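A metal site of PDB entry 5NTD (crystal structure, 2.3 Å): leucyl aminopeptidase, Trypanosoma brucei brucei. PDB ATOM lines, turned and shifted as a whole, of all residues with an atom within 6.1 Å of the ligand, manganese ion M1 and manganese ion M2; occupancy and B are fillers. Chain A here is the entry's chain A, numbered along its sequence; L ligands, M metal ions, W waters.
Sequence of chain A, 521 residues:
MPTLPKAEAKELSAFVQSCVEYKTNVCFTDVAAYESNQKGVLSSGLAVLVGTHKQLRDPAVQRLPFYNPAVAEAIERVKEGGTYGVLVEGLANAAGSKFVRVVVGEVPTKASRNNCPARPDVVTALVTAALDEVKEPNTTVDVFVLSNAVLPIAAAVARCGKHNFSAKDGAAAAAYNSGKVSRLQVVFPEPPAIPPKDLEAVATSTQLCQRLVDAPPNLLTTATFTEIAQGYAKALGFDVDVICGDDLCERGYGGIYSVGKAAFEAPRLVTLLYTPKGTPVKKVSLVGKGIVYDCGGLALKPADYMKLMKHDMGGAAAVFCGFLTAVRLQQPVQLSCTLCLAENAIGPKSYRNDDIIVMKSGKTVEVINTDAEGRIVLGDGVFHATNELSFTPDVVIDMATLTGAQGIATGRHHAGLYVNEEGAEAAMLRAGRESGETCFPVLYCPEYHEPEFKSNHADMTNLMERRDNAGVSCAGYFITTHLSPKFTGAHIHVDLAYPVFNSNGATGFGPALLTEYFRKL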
ATOM      1  N   LYS A 289      -5.126 -21.554   6.918  1.00  0.00           N
ATOM      2  CA  LYS A 289      -4.753 -22.361   8.137  1.00  0.00           C
ATOM      3  C   LYS A 289      -6.006 -22.982   8.674  1.00  0.00           C
ATOM      4  O   LYS A 289      -6.874 -22.292   9.211  1.00  0.00           O
ATOM      5  CB  LYS A 289      -4.029 -21.504   9.233  1.00  0.00           C
ATOM      6  CG  LYS A 289      -3.685 -22.253  10.506  1.00  0.00           C
ATOM      7  CD  LYS A 289      -3.181 -21.344  11.639  1.00  0.00           C
ATOM      8  CE  LYS A 289      -2.915 -22.104  12.960  1.00  0.00           C
ATOM      9  NZ  LYS A 289      -2.415 -21.366  14.172  1.00  0.00           N
ATOM     10  N   ILE A 291      -6.450 -25.300  11.244  1.00  0.00           N
ATOM     11  CA  ILE A 291      -6.162 -26.044  12.492  1.00  0.00           C
ATOM     12  C   ILE A 291      -7.469 -26.127  13.298  1.00  0.00           C
ATOM     13  O   ILE A 291      -7.876 -25.190  13.952  1.00  0.00           O
ATOM     14  CB  ILE A 291      -5.012 -25.445  13.301  1.00  0.00           C
ATOM     15  CG1 ILE A 291      -3.746 -25.460  12.468  1.00  0.00           C
ATOM     16  CG2 ILE A 291      -4.819 -26.227  14.594  1.00  0.00           C
ATOM     17  CD1 ILE A 291      -3.270 -26.824  12.019  1.00  0.00           C
ATOM     18  N   ASP A 294      -6.063 -26.350  18.201  1.00  0.00           N
ATOM     19  CA  ASP A 294      -4.637 -26.111  18.485  1.00  0.00           C
ATOM     20  C   ASP A 294      -4.454 -26.327  20.018  1.00  0.00           C
ATOM     21  O   ASP A 294      -4.603 -25.398  20.797  1.00  0.00           O
ATOM     22  CB  ASP A 294      -4.207 -24.677  18.079  1.00  0.00           C
ATOM     23  CG  ASP A 294      -2.680 -24.443  18.113  1.00  0.00           C
ATOM     24  OD1 ASP A 294      -1.998 -25.449  18.430  1.00  0.00           O
ATOM     25  OD2 ASP A 294      -2.134 -23.311  17.694  1.00  0.00           O
ATOM     26  N   GLY A 296      -1.600 -26.988  21.129  1.00  0.00           N
ATOM     27  CA  GLY A 296      -0.164 -26.687  21.253  1.00  0.00           C
ATOM     28  C   GLY A 296       0.792 -27.837  20.901  1.00  0.00           C
ATOM     29  O   GLY A 296       1.974 -27.626  20.664  1.00  0.00           O
ATOM     30  N   LYS A 301      -0.497 -25.873  25.465  1.00  0.00           N
ATOM     31  CA  LYS A 301      -1.043 -24.607  25.947  1.00  0.00           C
ATOM     32  C   LYS A 301      -1.656 -24.781  27.334  1.00  0.00           C
ATOM     33  O   LYS A 301      -2.299 -25.793  27.594  1.00  0.00           O
ATOM     34  CB  LYS A 301      -2.133 -24.084  25.042  1.00  0.00           C
ATOM     35  CG  LYS A 301      -1.662 -23.721  23.661  1.00  0.00           C
ATOM     36  CD  LYS A 301      -2.813 -23.132  22.851  1.00  0.00           C
ATOM     37  CE  LYS A 301      -2.381 -22.822  21.440  1.00  0.00           C
ATOM     38  NZ  LYS A 301      -1.396 -21.721  21.424  1.00  0.00           N
ATOM     39  N   MET A 309      -9.328 -22.116  20.871  1.00  0.00           N
ATOM     40  CA  MET A 309      -8.503 -22.653  19.761  1.00  0.00           C
ATOM     41  C   MET A 309      -9.292 -23.486  18.725  1.00  0.00           C
ATOM     42  O   MET A 309      -8.768 -23.889  17.717  1.00  0.00           O
ATOM     43  CB  MET A 309      -7.272 -23.398  20.262  1.00  0.00           C
ATOM     44  CG  MET A 309      -6.277 -22.459  20.944  1.00  0.00           C
ATOM     45  SD  MET A 309      -5.612 -21.212  19.804  1.00  0.00           S
ATOM     46  CE  MET A 309      -5.673 -19.739  20.823  1.00  0.00           C
ATOM     47  N   ASP A 312      -9.123 -21.764  15.475  1.00  0.00           N
ATOM     48  CA  ASP A 312      -7.820 -21.799  14.793  1.00  0.00           C
ATOM     49  C   ASP A 312      -7.911 -22.264  13.343  1.00  0.00           C
ATOM     50  O   ASP A 312      -6.905 -22.368  12.641  1.00  0.00           O
ATOM     51  CB  ASP A 312      -6.786 -22.668  15.564  1.00  0.00           C
ATOM     52  CG  ASP A 312      -5.355 -22.096  15.483  1.00  0.00           C
ATOM     53  OD1 ASP A 312      -5.240 -20.874  15.298  1.00  0.00           O
ATOM     54  OD2 ASP A 312      -4.340 -22.848  15.632  1.00  0.00           O
ATOM     55  N   ASN A 344      -3.796 -30.109  15.820  1.00  0.00           N
ATOM     56  CA  ASN A 344      -2.514 -30.102  16.572  1.00  0.00           C
ATOM     57  C   ASN A 344      -2.756 -30.754  17.922  1.00  0.00           C
ATOM     58  O   ASN A 344      -3.161 -30.109  18.878  1.00  0.00           O
ATOM     59  CB  ASN A 344      -1.964 -28.694  16.743  1.00  0.00           C
ATOM     60  CG  ASN A 344      -0.477 -28.689  17.133  1.00  0.00           C
ATOM     61  OD1 ASN A 344       0.216 -29.678  16.965  1.00  0.00           O
ATOM     62  ND2 ASN A 344       0.004 -27.544  17.592  1.00  0.00           N
ATOM     63  N   ASN A 369       9.387 -25.329  18.651  1.00  0.00           N
ATOM     64  CA  ASN A 369       8.155 -25.271  19.391  1.00  0.00           C
ATOM     65  C   ASN A 369       7.001 -25.769  18.549  1.00  0.00           C
ATOM     66  O   ASN A 369       6.641 -25.170  17.538  1.00  0.00           O
ATOM     67  CB  ASN A 369       7.907 -23.840  19.867  1.00  0.00           C
ATOM     68  CG  ASN A 369       6.792 -23.752  20.893  1.00  0.00           C
ATOM     69  OD1 ASN A 369       5.680 -24.230  20.669  1.00  0.00           O
ATOM     70  ND2 ASN A 369       7.079 -23.122  22.017  1.00  0.00           N
ATOM     71  N   THR A 370       6.344 -26.817  19.027  1.00  0.00           N
ATOM     72  CA  THR A 370       5.246 -27.459  18.292  1.00  0.00           C
ATOM     73  C   THR A 370       3.988 -26.626  18.213  1.00  0.00           C
ATOM     74  O   THR A 370       3.104 -26.899  17.419  1.00  0.00           O
ATOM     75  CB  THR A 370       4.853 -28.803  18.888  1.00  0.00           C
ATOM     76  OG1 THR A 370       4.473 -28.646  20.247  1.00  0.00           O
ATOM     77  CG2 THR A 370       5.989 -29.812  18.760  1.00  0.00           C
ATOM     78  N   ASP A 371       3.912 -25.624  19.064  1.00  0.00           N
ATOM     79  CA  ASP A 371       2.758 -24.686  19.093  1.00  0.00           C
ATOM     80  C   ASP A 371       2.823 -23.533  18.051  1.00  0.00           C
ATOM     81  O   ASP A 371       1.809 -22.817  17.840  1.00  0.00           O
ATOM     82  CB  ASP A 371       2.555 -24.097  20.472  1.00  0.00           C
ATOM     83  CG  ASP A 371       1.159 -23.534  20.671  1.00  0.00           C
ATOM     84  OD1 ASP A 371       0.232 -23.720  19.796  1.00  0.00           O
ATOM     85  OD2 ASP A 371       1.030 -22.825  21.687  1.00  0.00           O
ATOM     86  N   ALA A 372       3.962 -23.475  17.390  1.00  0.00           N
ATOM     87  CA  ALA A 372       4.131 -22.735  16.116  1.00  0.00           C
ATOM     88  C   ALA A 372       3.904 -23.660  14.887  1.00  0.00           C
ATOM     89  O   ALA A 372       4.738 -23.820  14.030  1.00  0.00           O
ATOM     90  CB  ALA A 372       5.473 -22.055  16.038  1.00  0.00           C
ATOM     91  N   GLU A 373       2.720 -24.213  14.860  1.00  0.00           N
ATOM     92  CA  GLU A 373       2.302 -25.251  13.890  1.00  0.00           C
ATOM     93  C   GLU A 373       1.754 -24.647  12.595  1.00  0.00           C
ATOM     94  O   GLU A 373       1.856 -25.219  11.529  1.00  0.00           O
ATOM     95  CB  GLU A 373       1.244 -26.176  14.506  1.00  0.00           C
ATOM     96  CG  GLU A 373      -0.220 -25.689  14.507  1.00  0.00           C
ATOM     97  CD  GLU A 373      -0.572 -24.497  15.404  1.00  0.00           C
ATOM     98  OE1 GLU A 373      -1.631 -23.819  15.122  1.00  0.00           O
ATOM     99  OE2 GLU A 373       0.122 -24.279  16.450  1.00  0.00           O
ATOM    100  N   GLY A 374       1.154 -23.480  12.734  1.00  0.00           N
ATOM    101  CA  GLY A 374       0.417 -22.857  11.637  1.00  0.00           C
ATOM    102  C   GLY A 374       1.320 -22.517  10.481  1.00  0.00           C
ATOM    103  O   GLY A 374       1.010 -22.811   9.337  1.00  0.00           O
ATOM    104  N   ARG A 375       2.464 -21.928  10.801  1.00  0.00           N
ATOM    105  CA  ARG A 375       3.387 -21.496   9.778  1.00  0.00           C
ATOM    106  C   ARG A 375       3.952 -22.711   9.000  1.00  0.00           C
ATOM    107  O   ARG A 375       4.220 -22.633   7.814  1.00  0.00           O
ATOM    108  CB  ARG A 375       4.492 -20.652  10.367  1.00  0.00           C
ATOM    109  CG  ARG A 375       5.491 -21.434  11.214  1.00  0.00           C
ATOM    110  CD  ARG A 375       6.336 -20.513  12.032  1.00  0.00           C
ATOM    111  NE  ARG A 375       5.539 -19.866  13.049  1.00  0.00           N
ATOM    112  CZ  ARG A 375       5.945 -18.834  13.754  1.00  0.00           C
ATOM    113  NH1 ARG A 375       7.168 -18.352  13.591  1.00  0.00           N
ATOM    114  NH2 ARG A 375       5.141 -18.266  14.622  1.00  0.00           N
ATOM    115  N   THR A 401      -5.054 -17.670  11.554  1.00  0.00           N
ATOM    116  CA  THR A 401      -5.123 -17.226  12.929  1.00  0.00           C
ATOM    117  C   THR A 401      -3.757 -17.533  13.576  1.00  0.00           C
ATOM    118  O   THR A 401      -3.613 -18.462  14.371  1.00  0.00           O
ATOM    119  CB  THR A 401      -6.243 -17.934  13.687  1.00  0.00           C
ATOM    120  OG1 THR A 401      -6.169 -19.341  13.443  1.00  0.00           O
ATOM    121  CG2 THR A 401      -7.587 -17.414  13.244  1.00  0.00           C
ATOM    122  N   LEU A 402      -2.763 -16.748  13.208  1.00  0.00           N
ATOM    123  CA  LEU A 402      -1.379 -17.235  13.317  1.00  0.00           C
ATOM    124  C   LEU A 402      -0.631 -16.905  14.605  1.00  0.00           C
ATOM    125  O   LEU A 402       0.110 -17.730  15.081  1.00  0.00           O
ATOM    126  CB  LEU A 402      -0.557 -16.823  12.097  1.00  0.00           C
ATOM    127  CG  LEU A 402       0.700 -17.682  11.863  1.00  0.00           C
ATOM    128  CD1 LEU A 402       0.370 -19.153  11.691  1.00  0.00           C
ATOM    129  CD2 LEU A 402       1.414 -17.182  10.622  1.00  0.00           C
ATOM    130  N   THR A 403      -0.759 -15.680  15.080  1.00  0.00           N
ATOM    131  CA  THR A 403       0.047 -15.225  16.198  1.00  0.00           C
ATOM    132  C   THR A 403      -0.714 -14.417  17.229  1.00  0.00           C
ATOM    133  O   THR A 403      -1.548 -13.604  16.880  1.00  0.00           O
ATOM    134  CB  THR A 403       1.246 -14.340  15.757  1.00  0.00           C
ATOM    135  OG1 THR A 403       0.776 -13.113  15.229  1.00  0.00           O
ATOM    136  CG2 THR A 403       2.121 -15.023  14.731  1.00  0.00           C
ATOM    137  N   GLY A 404      -0.341 -14.612  18.478  1.00  0.00           N
ATOM    138  CA  GLY A 404      -0.777 -13.712  19.564  1.00  0.00           C
ATOM    139  C   GLY A 404      -0.248 -12.313  19.392  1.00  0.00           C
ATOM    140  O   GLY A 404      -0.882 -11.327  19.706  1.00  0.00           O
ATOM    141  N   ALA A 405       0.948 -12.239  18.822  1.00  0.00           N
ATOM    142  CA  ALA A 405       1.557 -10.945  18.452  1.00  0.00           C
ATOM    143  C   ALA A 405       0.609 -10.053  17.593  1.00  0.00           C
ATOM    144  O   ALA A 405       0.630  -8.860  17.687  1.00  0.00           O
ATOM    145  CB  ALA A 405       2.865 -11.168  17.699  1.00  0.00           C
ATOM    146  N   LEU A 463      10.737 -21.134  14.742  1.00  0.00           N
ATOM    147  CA  LEU A 463      10.521 -20.111  15.772  1.00  0.00           C
ATOM    148  C   LEU A 463      11.699 -19.197  15.917  1.00  0.00           C
ATOM    149  O   LEU A 463      12.822 -19.614  15.954  1.00  0.00           O
ATOM    150  CB  LEU A 463      10.214 -20.747  17.135  1.00  0.00           C
ATOM    151  CG  LEU A 463       9.712 -19.786  18.209  1.00  0.00           C
ATOM    152  CD1 LEU A 463       8.293 -19.323  17.907  1.00  0.00           C
ATOM    153  CD2 LEU A 463       9.719 -20.412  19.587  1.00  0.00           C
ATOM    154  N   ARG A 467      11.784 -13.323  20.330  1.00  0.00           N
ATOM    155  CA  ARG A 467      10.341 -13.197  20.067  1.00  0.00           C
ATOM    156  C   ARG A 467       9.837 -11.756  20.119  1.00  0.00           C
ATOM    157  O   ARG A 467       8.724 -11.460  19.708  1.00  0.00           O
ATOM    158  CB  ARG A 467       9.562 -14.069  21.031  1.00  0.00           C
ATOM    159  CG  ARG A 467       9.957 -15.542  20.887  1.00  0.00           C
ATOM    160  CD  ARG A 467       8.926 -16.440  20.254  1.00  0.00           C
ATOM    161  NE  ARG A 467       7.529 -16.107  20.444  1.00  0.00           N
ATOM    162  CZ  ARG A 467       6.794 -16.524  21.464  1.00  0.00           C
ATOM    163  NH1 ARG A 467       5.529 -16.159  21.526  1.00  0.00           N
ATOM    164  NH2 ARG A 467       7.350 -17.282  22.420  1.00  0.00           N
ATOM    165  N   ALA A 497      -5.733 -13.685  13.637  1.00  0.00           N
ATOM    166  CA  ALA A 497      -5.878 -14.366  14.969  1.00  0.00           C
ATOM    167  C   ALA A 497      -7.041 -13.834  15.813  1.00  0.00           C
ATOM    168  O   ALA A 497      -7.897 -14.582  16.227  1.00  0.00           O
ATOM    169  CB  ALA A 497      -4.609 -14.261  15.774  1.00  0.00           C
ATOM    170  N   TYR A 498      -7.114 -12.536  15.953  1.00  0.00           N
ATOM    171  CA  TYR A 498      -8.189 -11.904  16.738  1.00  0.00           C
ATOM    172  C   TYR A 498      -9.453 -11.419  15.988  1.00  0.00           C
ATOM    173  O   TYR A 498     -10.551 -11.504  16.523  1.00  0.00           O
ATOM    174  CB  TYR A 498      -7.610 -10.777  17.579  1.00  0.00           C
ATOM    175  CG  TYR A 498      -6.734 -11.307  18.685  1.00  0.00           C
ATOM    176  CD1 TYR A 498      -5.400 -11.618  18.458  1.00  0.00           C
ATOM    177  CD2 TYR A 498      -7.271 -11.570  19.966  1.00  0.00           C
ATOM    178  CE1 TYR A 498      -4.608 -12.118  19.464  1.00  0.00           C
ATOM    179  CE2 TYR A 498      -6.493 -12.088  20.973  1.00  0.00           C
ATOM    180  CZ  TYR A 498      -5.157 -12.359  20.727  1.00  0.00           C
ATOM    181  OH  TYR A 498      -4.369 -12.868  21.731  1.00  0.00           O
ATOM    182  N   PHE A 501     -13.000 -13.422  15.838  1.00  0.00           N
ATOM    183  CA  PHE A 501     -13.901 -13.607  16.962  1.00  0.00           C
ATOM    184  C   PHE A 501     -14.077 -12.368  17.804  1.00  0.00           C
ATOM    185  O   PHE A 501     -13.277 -11.474  17.799  1.00  0.00           O
ATOM    186  CB  PHE A 501     -13.484 -14.805  17.816  1.00  0.00           C
ATOM    187  CG  PHE A 501     -12.330 -14.504  18.747  1.00  0.00           C
ATOM    188  CD1 PHE A 501     -11.011 -14.571  18.306  1.00  0.00           C
ATOM    189  CD2 PHE A 501     -12.572 -14.189  20.088  1.00  0.00           C
ATOM    190  CE1 PHE A 501      -9.958 -14.319  19.158  1.00  0.00           C
ATOM    191  CE2 PHE A 501     -11.509 -13.946  20.955  1.00  0.00           C
ATOM    192  CZ  PHE A 501     -10.200 -13.987  20.482  1.00  0.00           C
HETATM  193  N1  LIG L   1      -2.992 -20.568  16.814  1.00  0.00           N
HETATM  194  C1  LIG L   1      -2.100 -19.834  17.681  1.00  0.00           C
HETATM  195  C2  LIG L   1      -2.205 -18.296  17.603  1.00  0.00           C
HETATM  196  C3  LIG L   1      -3.250 -17.555  18.430  1.00  0.00           C
HETATM  197  C4  LIG L   1      -4.562 -17.466  18.012  1.00  0.00           C
HETATM  198  C5  LIG L   1      -2.891 -16.863  19.594  1.00  0.00           C
HETATM  199  C6  LIG L   1      -5.482 -16.740  18.757  1.00  0.00           C
HETATM  200  C7  LIG L   1      -3.837 -16.162  20.342  1.00  0.00           C
HETATM  201  C8  LIG L   1      -5.158 -16.094  19.931  1.00  0.00           C
HETATM  202  C9  LIG L   1      -0.723 -20.299  17.212  1.00  0.00           C
HETATM  203  O1  LIG L   1      -0.829 -21.675  16.760  1.00  0.00           O
HETATM  204  C10 LIG L   1       0.192 -20.307  18.377  1.00  0.00           C
HETATM  205  O2  LIG L   1       0.182 -21.369  19.000  1.00  0.00           O
HETATM  206  N2  LIG L   1       0.908 -19.202  18.553  1.00  0.00           N
HETATM  207  C11 LIG L   1       1.890 -18.987  19.582  1.00  0.00           C
HETATM  208  C12 LIG L   1       3.279 -19.508  19.168  1.00  0.00           C
HETATM  209  C13 LIG L   1       4.276 -19.668  20.308  1.00  0.00           C
HETATM  210  C14 LIG L   1       3.749 -20.372  21.571  1.00  0.00           C
HETATM  211  C15 LIG L   1       5.481 -20.450  19.831  1.00  0.00           C
HETATM  212  C16 LIG L   1       2.012 -17.526  19.896  1.00  0.00           C
HETATM  213  O3  LIG L   1       1.704 -16.739  18.999  1.00  0.00           O
HETATM  214  O4  LIG L   1       2.408 -17.146  21.028  1.00  0.00           O
HETATM  215 MN    MN M   1      -0.155 -23.048  18.008  1.00  0.00          MN
HETATM  216 MN    MN M   2      -2.511 -22.331  15.968  1.00  0.00          MN
HETATM  217  O   HOH W   1       3.072 -14.347  18.946  1.00  0.00           O
HETATM  218  O   HOH W   2      -7.034 -19.254  16.932  1.00  0.00           O
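Of the 25 residues printed, 4 come within 4 Å of manganese ion M2.
The nearest printed residue that does not touch manganese ion M2 is Thr 401 (4.3 Å).
The side-chain carboxylate of Asp 294 sits at hydrogen-bond distance from the backbone NH of Gly 296 (3.1 Å).
O of Thr 401 lies close to NZ of Lys 289 (3.1 Å).
N of Asp 371 lies within hydrogen-bond range of O of Gly 296 (3.2 Å).
The side-chain carboxylate (OD1) of Asp 294 is in hydrogen-bond range of the side-chain amide nitrogen (ND2) of Asn 344 (3.0 Å).
The side-chain amino group (NZ) of Lys 301 is in salt-bridge range of the side-chain carboxylate (OD2) of Asp 371, 2.7 Å away.
O of Asp 312 lies within hydrogen-bond range of N of Ile 291 (3.3 Å).
The backbone NH (N) of Asp 371 sits at hydrogen-bond distance from the side-chain amide oxygen (OD1) of Asn 369.
The side-chain hydroxyl (OG1) of Thr 401 is in hydrogen-bond range of the side-chain carboxylate (OD1) of Asp 312 (2.6 Å).
NZ of Lys 301 touches manganese ion M1, 3.9 Å away.
Within 4 Å of manganese ion M1: Asp 294, Lys 301, Asp 371 and Glu 373.
CE of Met 309 touches C6 of the ligand, 3.6 Å away.
CG of Asn 369 touches C15 of the ligand, at 3.7 Å.
Leu 402 touches the ligand.
Thr 403 touches the ligand (CA to O3, 3.6 Å).
Leu 463 touches the ligand.
CB of Ala 497 touches C4 of the ligand, 3.9 Å away.
Tyr 498 touches the ligand (OH to C7, 3.6 Å).
Within 4 Å of the ligand: Lys 289, Asp 294, Lys 301, Met 309, Asp 312, Asn 369, Asp 371, Glu 373, Thr 401, Leu 402, Thr 403, Gly 404, Leu 463, Arg 467, Ala 497 and Tyr 498.
OE1 of Glu 373 is bound to manganese ion M2 (1.9 Å).
Manganese ion M2 is bound by OD2 of Asp 312, at 1.9 Å.
An oxygen (O1) of the ligand binds manganese ion M2.
Manganese ion M2 is bound by N1 of the ligand (2.0 Å).
Manganese ion M2 is bound by OD2 of Asp 294 (2.0 Å).
NZ of Lys 289 binds manganese ion M2, 2.0 Å away.
Manganese ion M2 has six donor atoms within binding distance.
NH1 of Arg 467 is in salt-bridge range of O4 of the ligand.
The backbone NH of Gly 404 lies within hydrogen-bond range of an oxygen (O3) of the ligand, at 3.0 Å.
NZ of Lys 301 lies close to O2 of the ligand (2.9 Å).
O of Thr 401 sits close to N1 of the ligand (3.3 Å).
Manganese ion M1 is bound by OD1 of Asp 371 (1.9 Å), O1 of the ligand (2.0 Å), O2 of the ligand (2.0 Å), O of Asp 371 (2.0 Å), OE2 of Glu 373 (2.0 Å) and OD2 of Asp 294 (2.0 Å).
Manganese ion M1 has six donor atoms within binding distance.
Water W1 lies within hydrogen-bond range of O3 of the ligand, N of Ala 405 and N of Gly 404.
Water W2 lies within hydrogen-bond range of the side-chain carboxylate of Asp 312 (2.9 Å) and the side-chain sulfur of Met 309 (3.8 Å).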
